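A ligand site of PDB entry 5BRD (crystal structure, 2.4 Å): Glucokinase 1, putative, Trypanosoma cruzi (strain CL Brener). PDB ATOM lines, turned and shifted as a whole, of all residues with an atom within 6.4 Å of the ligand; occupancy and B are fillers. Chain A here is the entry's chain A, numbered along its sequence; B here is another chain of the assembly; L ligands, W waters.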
ATOM      1  N   VAL A 105      -6.573  14.942 -21.222  1.00  0.00           N
ATOM      2  CA  VAL A 105      -7.527  15.297 -22.278  1.00  0.00           C
ATOM      3  C   VAL A 105      -8.804  14.437 -22.183  1.00  0.00           C
ATOM      4  O   VAL A 105      -8.774  13.343 -21.627  1.00  0.00           O
ATOM      5  CB  VAL A 105      -6.874  15.139 -23.671  1.00  0.00           C
ATOM      6  CG1 VAL A 105      -5.665  16.074 -23.811  1.00  0.00           C
ATOM      7  CG2 VAL A 105      -6.458  13.688 -23.932  1.00  0.00           C
ATOM      8  N   PRO A 106      -9.944  14.932 -22.694  1.00  0.00           N
ATOM      9  CA  PRO A 106     -11.203  14.192 -22.488  1.00  0.00           C
ATOM     10  C   PRO A 106     -11.572  13.150 -23.554  1.00  0.00           C
ATOM     11  O   PRO A 106     -12.659  13.216 -24.096  1.00  0.00           O
ATOM     12  CB  PRO A 106     -12.249  15.302 -22.506  1.00  0.00           C
ATOM     13  CG  PRO A 106     -11.667  16.330 -23.400  1.00  0.00           C
ATOM     14  CD  PRO A 106     -10.185  16.302 -23.178  1.00  0.00           C
ATOM     15  N   GLY A 107     -10.696  12.189 -23.823  1.00  0.00           N
ATOM     16  CA  GLY A 107     -10.980  11.133 -24.775  1.00  0.00           C
ATOM     17  C   GLY A 107     -10.058   9.952 -24.496  1.00  0.00           C
ATOM     18  O   GLY A 107      -9.260  10.011 -23.572  1.00  0.00           O
ATOM     19  N   PRO A 108     -10.174   8.876 -25.280  1.00  0.00           N
ATOM     20  CA  PRO A 108      -9.226   7.758 -25.128  1.00  0.00           C
ATOM     21  C   PRO A 108      -7.790   8.164 -25.512  1.00  0.00           C
ATOM     22  O   PRO A 108      -7.581   8.886 -26.495  1.00  0.00           O
ATOM     23  CB  PRO A 108      -9.764   6.710 -26.106  1.00  0.00           C
ATOM     24  CG  PRO A 108     -11.223   7.061 -26.275  1.00  0.00           C
ATOM     25  CD  PRO A 108     -11.274   8.560 -26.204  1.00  0.00           C
ATOM     26  N   GLY A 116      -7.346  10.800 -28.626  1.00  0.00           N
ATOM     27  CA  GLY A 116      -8.406  10.912 -29.613  1.00  0.00           C
ATOM     28  C   GLY A 116      -8.991   9.551 -29.953  1.00  0.00           C
ATOM     29  O   GLY A 116      -8.389   8.514 -29.643  1.00  0.00           O
ATOM     30  N   PRO A 117     -10.185   9.544 -30.585  1.00  0.00           N
ATOM     31  CA  PRO A 117     -10.917  10.736 -31.008  1.00  0.00           C
ATOM     32  C   PRO A 117     -11.662  11.355 -29.832  1.00  0.00           C
ATOM     33  O   PRO A 117     -11.847  10.670 -28.823  1.00  0.00           O
ATOM     34  CB  PRO A 117     -11.917  10.174 -32.010  1.00  0.00           C
ATOM     35  CG  PRO A 117     -12.268   8.829 -31.439  1.00  0.00           C
ATOM     36  CD  PRO A 117     -10.973   8.306 -30.818  1.00  0.00           C
ATOM     37  N   PHE A 118     -12.107  12.601 -29.947  1.00  0.00           N
ATOM     38  CA  PHE A 118     -12.809  13.251 -28.841  1.00  0.00           C
ATOM     39  C   PHE A 118     -14.296  13.513 -29.108  1.00  0.00           C
ATOM     40  O   PHE A 118     -14.658  14.018 -30.166  1.00  0.00           O
ATOM     41  CB  PHE A 118     -12.110  14.559 -28.506  1.00  0.00           C
ATOM     42  CG  PHE A 118     -10.710  14.381 -28.004  1.00  0.00           C
ATOM     43  CD1 PHE A 118     -10.472  14.099 -26.669  1.00  0.00           C
ATOM     44  CD2 PHE A 118      -9.631  14.509 -28.858  1.00  0.00           C
ATOM     45  CE1 PHE A 118      -9.189  13.943 -26.192  1.00  0.00           C
ATOM     46  CE2 PHE A 118      -8.340  14.350 -28.393  1.00  0.00           C
ATOM     47  CZ  PHE A 118      -8.126  14.063 -27.064  1.00  0.00           C
ATOM     48  N   ASN A 119     -15.151  13.181 -28.142  1.00  0.00           N
ATOM     49  CA  ASN A 119     -16.590  13.468 -28.255  1.00  0.00           C
ATOM     50  C   ASN A 119     -16.882  14.981 -28.296  1.00  0.00           C
ATOM     51  O   ASN A 119     -17.872  15.393 -28.903  1.00  0.00           O
ATOM     52  CB  ASN A 119     -17.432  12.821 -27.135  1.00  0.00           C
ATOM     53  CG  ASN A 119     -17.808  11.349 -27.420  1.00  0.00           C
ATOM     54  OD1 ASN A 119     -17.935  10.930 -28.567  1.00  0.00           O
ATOM     55  ND2 ASN A 119     -18.010  10.566 -26.348  1.00  0.00           N
ATOM     56  N   ASN A 120     -16.030  15.787 -27.666  1.00  0.00           N
ATOM     57  CA  ASN A 120     -16.217  17.250 -27.659  1.00  0.00           C
ATOM     58  C   ASN A 120     -15.530  17.947 -28.817  1.00  0.00           C
ATOM     59  O   ASN A 120     -16.164  18.633 -29.618  1.00  0.00           O
ATOM     60  CB  ASN A 120     -15.634  17.889 -26.391  1.00  0.00           C
ATOM     61  CG  ASN A 120     -15.898  17.081 -25.152  1.00  0.00           C
ATOM     62  OD1 ASN A 120     -15.059  16.276 -24.735  1.00  0.00           O
ATOM     63  ND2 ASN A 120     -17.061  17.311 -24.528  1.00  0.00           N
ATOM     64  N   ASN A 144      -5.685  10.282 -20.083  1.00  0.00           N
ATOM     65  CA  ASN A 144      -7.143  10.452 -20.133  1.00  0.00           C
ATOM     66  C   ASN A 144      -7.615  11.264 -18.889  1.00  0.00           C
ATOM     67  O   ASN A 144      -7.023  11.173 -17.822  1.00  0.00           O
ATOM     68  CB  ASN A 144      -7.843   9.087 -20.233  1.00  0.00           C
ATOM     69  CG  ASN A 144      -9.346   9.142 -19.907  1.00  0.00           C
ATOM     70  OD1 ASN A 144      -9.769   8.831 -18.799  1.00  0.00           O
ATOM     71  ND2 ASN A 144     -10.155   9.480 -20.903  1.00  0.00           N
ATOM     72  N   ASP A 145      -8.632  12.090 -19.042  1.00  0.00           N
ATOM     73  CA  ASP A 145      -9.053  12.940 -17.932  1.00  0.00           C
ATOM     74  C   ASP A 145      -9.374  12.165 -16.650  1.00  0.00           C
ATOM     75  O   ASP A 145      -9.044  12.624 -15.566  1.00  0.00           O
ATOM     76  CB  ASP A 145     -10.186  13.905 -18.313  1.00  0.00           C
ATOM     77  CG  ASP A 145     -11.483  13.210 -18.742  1.00  0.00           C
ATOM     78  OD1 ASP A 145     -11.536  11.973 -18.908  1.00  0.00           O
ATOM     79  OD2 ASP A 145     -12.483  13.950 -18.931  1.00  0.00           O
ATOM     80  N   LEU A 146      -9.952  10.980 -16.783  1.00  0.00           N
ATOM     81  CA  LEU A 146     -10.300  10.187 -15.608  1.00  0.00           C
ATOM     82  C   LEU A 146      -9.138   9.351 -15.119  1.00  0.00           C
ATOM     83  O   LEU A 146      -9.135   8.928 -13.961  1.00  0.00           O
ATOM     84  CB  LEU A 146     -11.535   9.321 -15.840  1.00  0.00           C
ATOM     85  CG  LEU A 146     -12.788   9.935 -15.219  1.00  0.00           C
ATOM     86  CD1 LEU A 146     -12.705   9.964 -13.681  1.00  0.00           C
ATOM     87  CD2 LEU A 146     -13.050  11.339 -15.780  1.00  0.00           C
ATOM     88  N   ALA A 196     -17.158   9.811 -13.111  1.00  0.00           N
ATOM     89  CA  ALA A 196     -17.366  11.256 -13.181  1.00  0.00           C
ATOM     90  C   ALA A 196     -18.554  11.599 -14.105  1.00  0.00           C
ATOM     91  O   ALA A 196     -18.362  11.830 -15.288  1.00  0.00           O
ATOM     92  CB  ALA A 196     -16.088  11.956 -13.648  1.00  0.00           C
ATOM     93  N   THR A 199     -20.474  16.312 -18.182  1.00  0.00           N
ATOM     94  CA  THR A 199     -20.901  16.517 -19.549  1.00  0.00           C
ATOM     95  C   THR A 199     -20.930  15.172 -20.265  1.00  0.00           C
ATOM     96  O   THR A 199     -21.978  14.752 -20.763  1.00  0.00           O
ATOM     97  CB  THR A 199     -19.948  17.488 -20.268  1.00  0.00           C
ATOM     98  OG1 THR A 199     -20.140  18.810 -19.730  1.00  0.00           O
ATOM     99  CG2 THR A 199     -20.221  17.507 -21.764  1.00  0.00           C
ATOM    100  N   GLY A 200     -19.776  14.509 -20.302  1.00  0.00           N
ATOM    101  CA  GLY A 200     -19.701  13.101 -20.632  1.00  0.00           C
ATOM    102  C   GLY A 200     -19.656  12.276 -19.348  1.00  0.00           C
ATOM    103  O   GLY A 200     -19.627  12.844 -18.259  1.00  0.00           O
ATOM    104  N   LEU A 201     -19.673  10.952 -19.463  1.00  0.00           N
ATOM    105  CA  LEU A 201     -19.524  10.083 -18.284  1.00  0.00           C
ATOM    106  C   LEU A 201     -18.107   9.454 -18.193  1.00  0.00           C
ATOM    107  O   LEU A 201     -17.773   8.557 -18.948  1.00  0.00           O
ATOM    108  CB  LEU A 201     -20.625   9.003 -18.282  1.00  0.00           C
ATOM    109  CG  LEU A 201     -20.605   7.882 -17.223  1.00  0.00           C
ATOM    110  CD1 LEU A 201     -20.756   8.412 -15.779  1.00  0.00           C
ATOM    111  CD2 LEU A 201     -21.645   6.792 -17.552  1.00  0.00           C
ATOM    112  N   GLY A 202     -17.268   9.933 -17.280  1.00  0.00           N
ATOM    113  CA  GLY A 202     -15.900   9.436 -17.156  1.00  0.00           C
ATOM    114  C   GLY A 202     -15.759   8.258 -16.206  1.00  0.00           C
ATOM    115  O   GLY A 202     -16.511   8.099 -15.259  1.00  0.00           O
ATOM    116  N   SER A 203     -14.785   7.401 -16.454  1.00  0.00           N
ATOM    117  CA  SER A 203     -14.601   6.233 -15.606  1.00  0.00           C
ATOM    118  C   SER A 203     -13.156   5.740 -15.559  1.00  0.00           C
ATOM    119  O   SER A 203     -12.527   5.553 -16.609  1.00  0.00           O
ATOM    120  CB  SER A 203     -15.486   5.100 -16.091  1.00  0.00           C
ATOM    121  OG  SER A 203     -15.053   4.631 -17.350  1.00  0.00           O
ATOM    122  N   LEU A 220     -10.765   3.577 -18.195  1.00  0.00           N
ATOM    123  CA  LEU A 220     -11.863   2.769 -18.710  1.00  0.00           C
ATOM    124  C   LEU A 220     -12.685   3.632 -19.621  1.00  0.00           C
ATOM    125  O   LEU A 220     -12.545   4.859 -19.576  1.00  0.00           O
ATOM    126  CB  LEU A 220     -12.747   2.253 -17.567  1.00  0.00           C
ATOM    127  CG  LEU A 220     -12.053   1.326 -16.559  1.00  0.00           C
ATOM    128  CD1 LEU A 220     -12.944   1.036 -15.369  1.00  0.00           C
ATOM    129  CD2 LEU A 220     -11.592   0.039 -17.236  1.00  0.00           C
ATOM    130  N   GLU A 221     -13.523   3.002 -20.445  1.00  0.00           N
ATOM    131  CA  GLU A 221     -14.599   3.693 -21.171  1.00  0.00           C
ATOM    132  C   GLU A 221     -15.948   3.002 -20.944  1.00  0.00           C
ATOM    133  O   GLU A 221     -16.618   2.581 -21.902  1.00  0.00           O
ATOM    134  CB  GLU A 221     -14.285   3.792 -22.680  1.00  0.00           C
ATOM    135  CG  GLU A 221     -13.122   4.700 -23.005  1.00  0.00           C
ATOM    136  CD  GLU A 221     -13.442   6.173 -22.805  1.00  0.00           C
ATOM    137  OE1 GLU A 221     -14.653   6.531 -22.751  1.00  0.00           O
ATOM    138  OE2 GLU A 221     -12.491   6.969 -22.709  1.00  0.00           O
ATOM    139  N   SER A 224     -19.413   3.960 -22.766  1.00  0.00           N
ATOM    140  CA  SER A 224     -19.733   3.614 -24.146  1.00  0.00           C
ATOM    141  C   SER A 224     -20.280   2.188 -24.301  1.00  0.00           C
ATOM    142  O   SER A 224     -20.671   1.782 -25.381  1.00  0.00           O
ATOM    143  CB  SER A 224     -18.530   3.839 -25.046  1.00  0.00           C
ATOM    144  OG  SER A 224     -18.171   5.196 -25.067  1.00  0.00           O
ATOM    145  N   GLU A 250     -23.571   6.502 -21.255  1.00  0.00           N
ATOM    146  CA  GLU A 250     -23.457   7.933 -21.416  1.00  0.00           C
ATOM    147  C   GLU A 250     -24.716   8.601 -22.052  1.00  0.00           C
ATOM    148  O   GLU A 250     -25.038   9.752 -21.714  1.00  0.00           O
ATOM    149  CB  GLU A 250     -22.190   8.313 -22.163  1.00  0.00           C
ATOM    150  CG  GLU A 250     -21.950   9.825 -22.155  1.00  0.00           C
ATOM    151  CD  GLU A 250     -20.598  10.223 -22.725  1.00  0.00           C
ATOM    152  OE1 GLU A 250     -20.501  10.482 -23.939  1.00  0.00           O
ATOM    153  OE2 GLU A 250     -19.635  10.277 -21.950  1.00  0.00           O
ATOM    154  N   MET B 309     -14.713  -2.006 -25.975  1.00  0.00           N
ATOM    155  CA  MET B 309     -14.970  -0.626 -25.688  1.00  0.00           C
ATOM    156  C   MET B 309     -14.631  -0.271 -24.229  1.00  0.00           C
ATOM    157  O   MET B 309     -13.916   0.686 -23.976  1.00  0.00           O
ATOM    158  CB  MET B 309     -16.432  -0.288 -26.000  1.00  0.00           C
ATOM    159  CG  MET B 309     -16.690   1.161 -25.875  1.00  0.00           C
ATOM    160  SD  MET B 309     -15.798   1.936 -27.219  1.00  0.00           S
ATOM    161  CE  MET B 309     -14.585   2.982 -26.396  1.00  0.00           C
ATOM    162  N   MET B 348     -20.183   1.667 -31.260  1.00  0.00           N
ATOM    163  CA  MET B 348     -18.897   2.346 -31.197  1.00  0.00           C
ATOM    164  C   MET B 348     -17.966   1.976 -32.367  1.00  0.00           C
ATOM    165  O   MET B 348     -16.928   2.615 -32.589  1.00  0.00           O
ATOM    166  CB  MET B 348     -18.233   2.126 -29.830  1.00  0.00           C
ATOM    167  CG  MET B 348     -18.929   2.877 -28.693  1.00  0.00           C
ATOM    168  SD  MET B 348     -19.216   4.593 -29.181  1.00  0.00           S
ATOM    169  CE  MET B 348     -19.916   5.362 -27.746  1.00  0.00           C
ATOM    170  N   PHE B 351     -16.475   4.380 -34.975  1.00  0.00           N
ATOM    171  CA  PHE B 351     -15.196   5.063 -34.757  1.00  0.00           C
ATOM    172  C   PHE B 351     -14.036   4.063 -34.792  1.00  0.00           C
ATOM    173  O   PHE B 351     -12.916   4.355 -34.374  1.00  0.00           O
ATOM    174  CB  PHE B 351     -15.210   5.800 -33.400  1.00  0.00           C
ATOM    175  CG  PHE B 351     -16.439   6.655 -33.169  1.00  0.00           C
ATOM    176  CD1 PHE B 351     -16.703   7.747 -33.981  1.00  0.00           C
ATOM    177  CD2 PHE B 351     -17.294   6.386 -32.119  1.00  0.00           C
ATOM    178  CE1 PHE B 351     -17.822   8.540 -33.764  1.00  0.00           C
ATOM    179  CE2 PHE B 351     -18.423   7.180 -31.901  1.00  0.00           C
ATOM    180  CZ  PHE B 351     -18.682   8.261 -32.725  1.00  0.00           C
ATOM    181  N   PHE B 353     -13.561   1.280 -33.005  1.00  0.00           N
ATOM    182  CA  PHE B 353     -13.097   0.740 -31.734  1.00  0.00           C
ATOM    183  C   PHE B 353     -13.066  -0.782 -31.638  1.00  0.00           C
ATOM    184  O   PHE B 353     -12.177  -1.348 -31.022  1.00  0.00           O
ATOM    185  CB  PHE B 353     -13.824   1.377 -30.542  1.00  0.00           C
ATOM    186  CG  PHE B 353     -13.210   2.652 -30.138  1.00  0.00           C
ATOM    187  CD1 PHE B 353     -12.190   2.669 -29.212  1.00  0.00           C
ATOM    188  CD2 PHE B 353     -13.607   3.836 -30.735  1.00  0.00           C
ATOM    189  CE1 PHE B 353     -11.585   3.853 -28.859  1.00  0.00           C
ATOM    190  CE2 PHE B 353     -13.013   5.033 -30.400  1.00  0.00           C
ATOM    191  CZ  PHE B 353     -12.000   5.041 -29.452  1.00  0.00           C
HETATM  192  C1  LIG L   1     -14.030   9.883 -21.910  1.00  0.00           C
HETATM  193  C2  LIG L   1     -15.010  10.355 -22.999  1.00  0.00           C
HETATM  194  C3  LIG L   1     -16.392  10.656 -22.439  1.00  0.00           C
HETATM  195  O1  LIG L   1     -16.209  11.711 -21.516  1.00  0.00           O
HETATM  196  C4  LIG L   1     -15.422  11.248 -20.365  1.00  0.00           C
HETATM  197  C5  LIG L   1     -14.012  10.812 -20.770  1.00  0.00           C
HETATM  198  N1  LIG L   1     -15.093   9.309 -23.994  1.00  0.00           N
HETATM  199  O2  LIG L   1     -13.389  10.116 -19.629  1.00  0.00           O
HETATM  200  O3  LIG L   1     -12.720   9.759 -22.482  1.00  0.00           O
HETATM  201  C6  LIG L   1     -15.379  12.363 -19.329  1.00  0.00           C
HETATM  202  O4  LIG L   1     -17.172  11.110 -23.458  1.00  0.00           O
HETATM  203  O5  LIG L   1     -14.700  13.483 -19.863  1.00  0.00           O
HETATM  204  C7  LIG L   1     -14.916   9.633 -25.284  1.00  0.00           C
HETATM  205  O6  LIG L   1     -14.691  10.774 -25.628  1.00  0.00           O
HETATM  206  C8  LIG L   1     -15.456   7.288 -25.950  1.00  0.00           C
HETATM  207  C9  LIG L   1     -14.933   8.524 -26.305  1.00  0.00           C
HETATM  208  C10 LIG L   1     -14.384   8.725 -27.545  1.00  0.00           C
HETATM  209  C11 LIG L   1     -14.373   7.704 -28.468  1.00  0.00           C
HETATM  210  C12 LIG L   1     -14.907   6.480 -28.131  1.00  0.00           C
HETATM  211  C13 LIG L   1     -15.447   6.267 -26.883  1.00  0.00           C
HETATM  212  O   HOH W   1     -17.418  15.433 -19.095  1.00  0.00           O
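The side-chain carboxylate of Glu 221 is in hydrogen-bond range of an oxygen (O3) of the ligand, at 2.8 Å.
The backbone NH (N) of Gly 107 lies close to an oxygen (O3) of the ligand (3.4 Å).
The side-chain amide nitrogen (ND2) of Asn 119 lies within hydrogen-bond range of an oxygen (O4) of the ligand (3.1 Å).
OE2 of Glu 250 is in hydrogen-bond range of O4 of the ligand, 3.0 Å away.
ND2 of Asn 144 sits at hydrogen-bond distance from O3 of the ligand (3.0 Å).
An oxygen (O5) of the ligand is in hydrogen-bond range of the side-chain carboxylate of Asp 145.
Water W1 lies within hydrogen-bond range of N of Gly 200 (2.8 Å), N of Thr 199 (3.3 Å) and O5 of the ligand (3.4 Å).
OE1 of Glu 250 lies within hydrogen-bond range of ND2 of Asn 119, 3.5 Å away.
The side-chain amide nitrogen (ND2) of Asn 144 is in hydrogen-bond range of the backbone carbonyl oxygen (O) of Gly 107.
O of Pro 108 sits at hydrogen-bond distance from N of Gly 116.
The backbone NH (N) of Ala 196 lies within hydrogen-bond range of the backbone carbonyl oxygen (O) of Gly 202, at 2.8 Å.
The backbone NH (N) of Asp 145 sits at hydrogen-bond distance from the backbone carbonyl oxygen (O) of Val 105, 2.9 Å away.
N of Leu 146 is in hydrogen-bond range of OD1 of Asn 144 (3.0 Å).
The side-chain amide nitrogen (ND2) of Asn 144 sits at hydrogen-bond distance from the side-chain carboxylate (OD1) of Asp 145.
N of Leu 201 is in hydrogen-bond range of OE2 of Glu 250 (2.6 Å).
Pro 106 touches the ligand.
Pro 108 touches the ligand.
Pro 117 touches the ligand (O to C10, 3.4 Å).
Gly 200 touches the ligand (CA to O1, 3.9 Å).
O of Leu 201 touches C4 of the ligand (3.8 Å).
CA of Gly 202 touches O2 of the ligand, at 3.6 Å.
OG of Ser 224 touches C13 of the ligand (3.4 Å).
Met 309 of chain B touches the ligand (CE to C13, 3.4 Å).
CE2 of Phe 353 of chain B touches C12 of the ligand, at 3.3 Å.
Hydrophobic or aromatic side chains that line the ligand: Pro 108, Pro 117, Met 309 of chain B and Phe 353 of chain B.
The nearest printed residue that does not touch the ligand is Leu 146 (4.1 Å).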
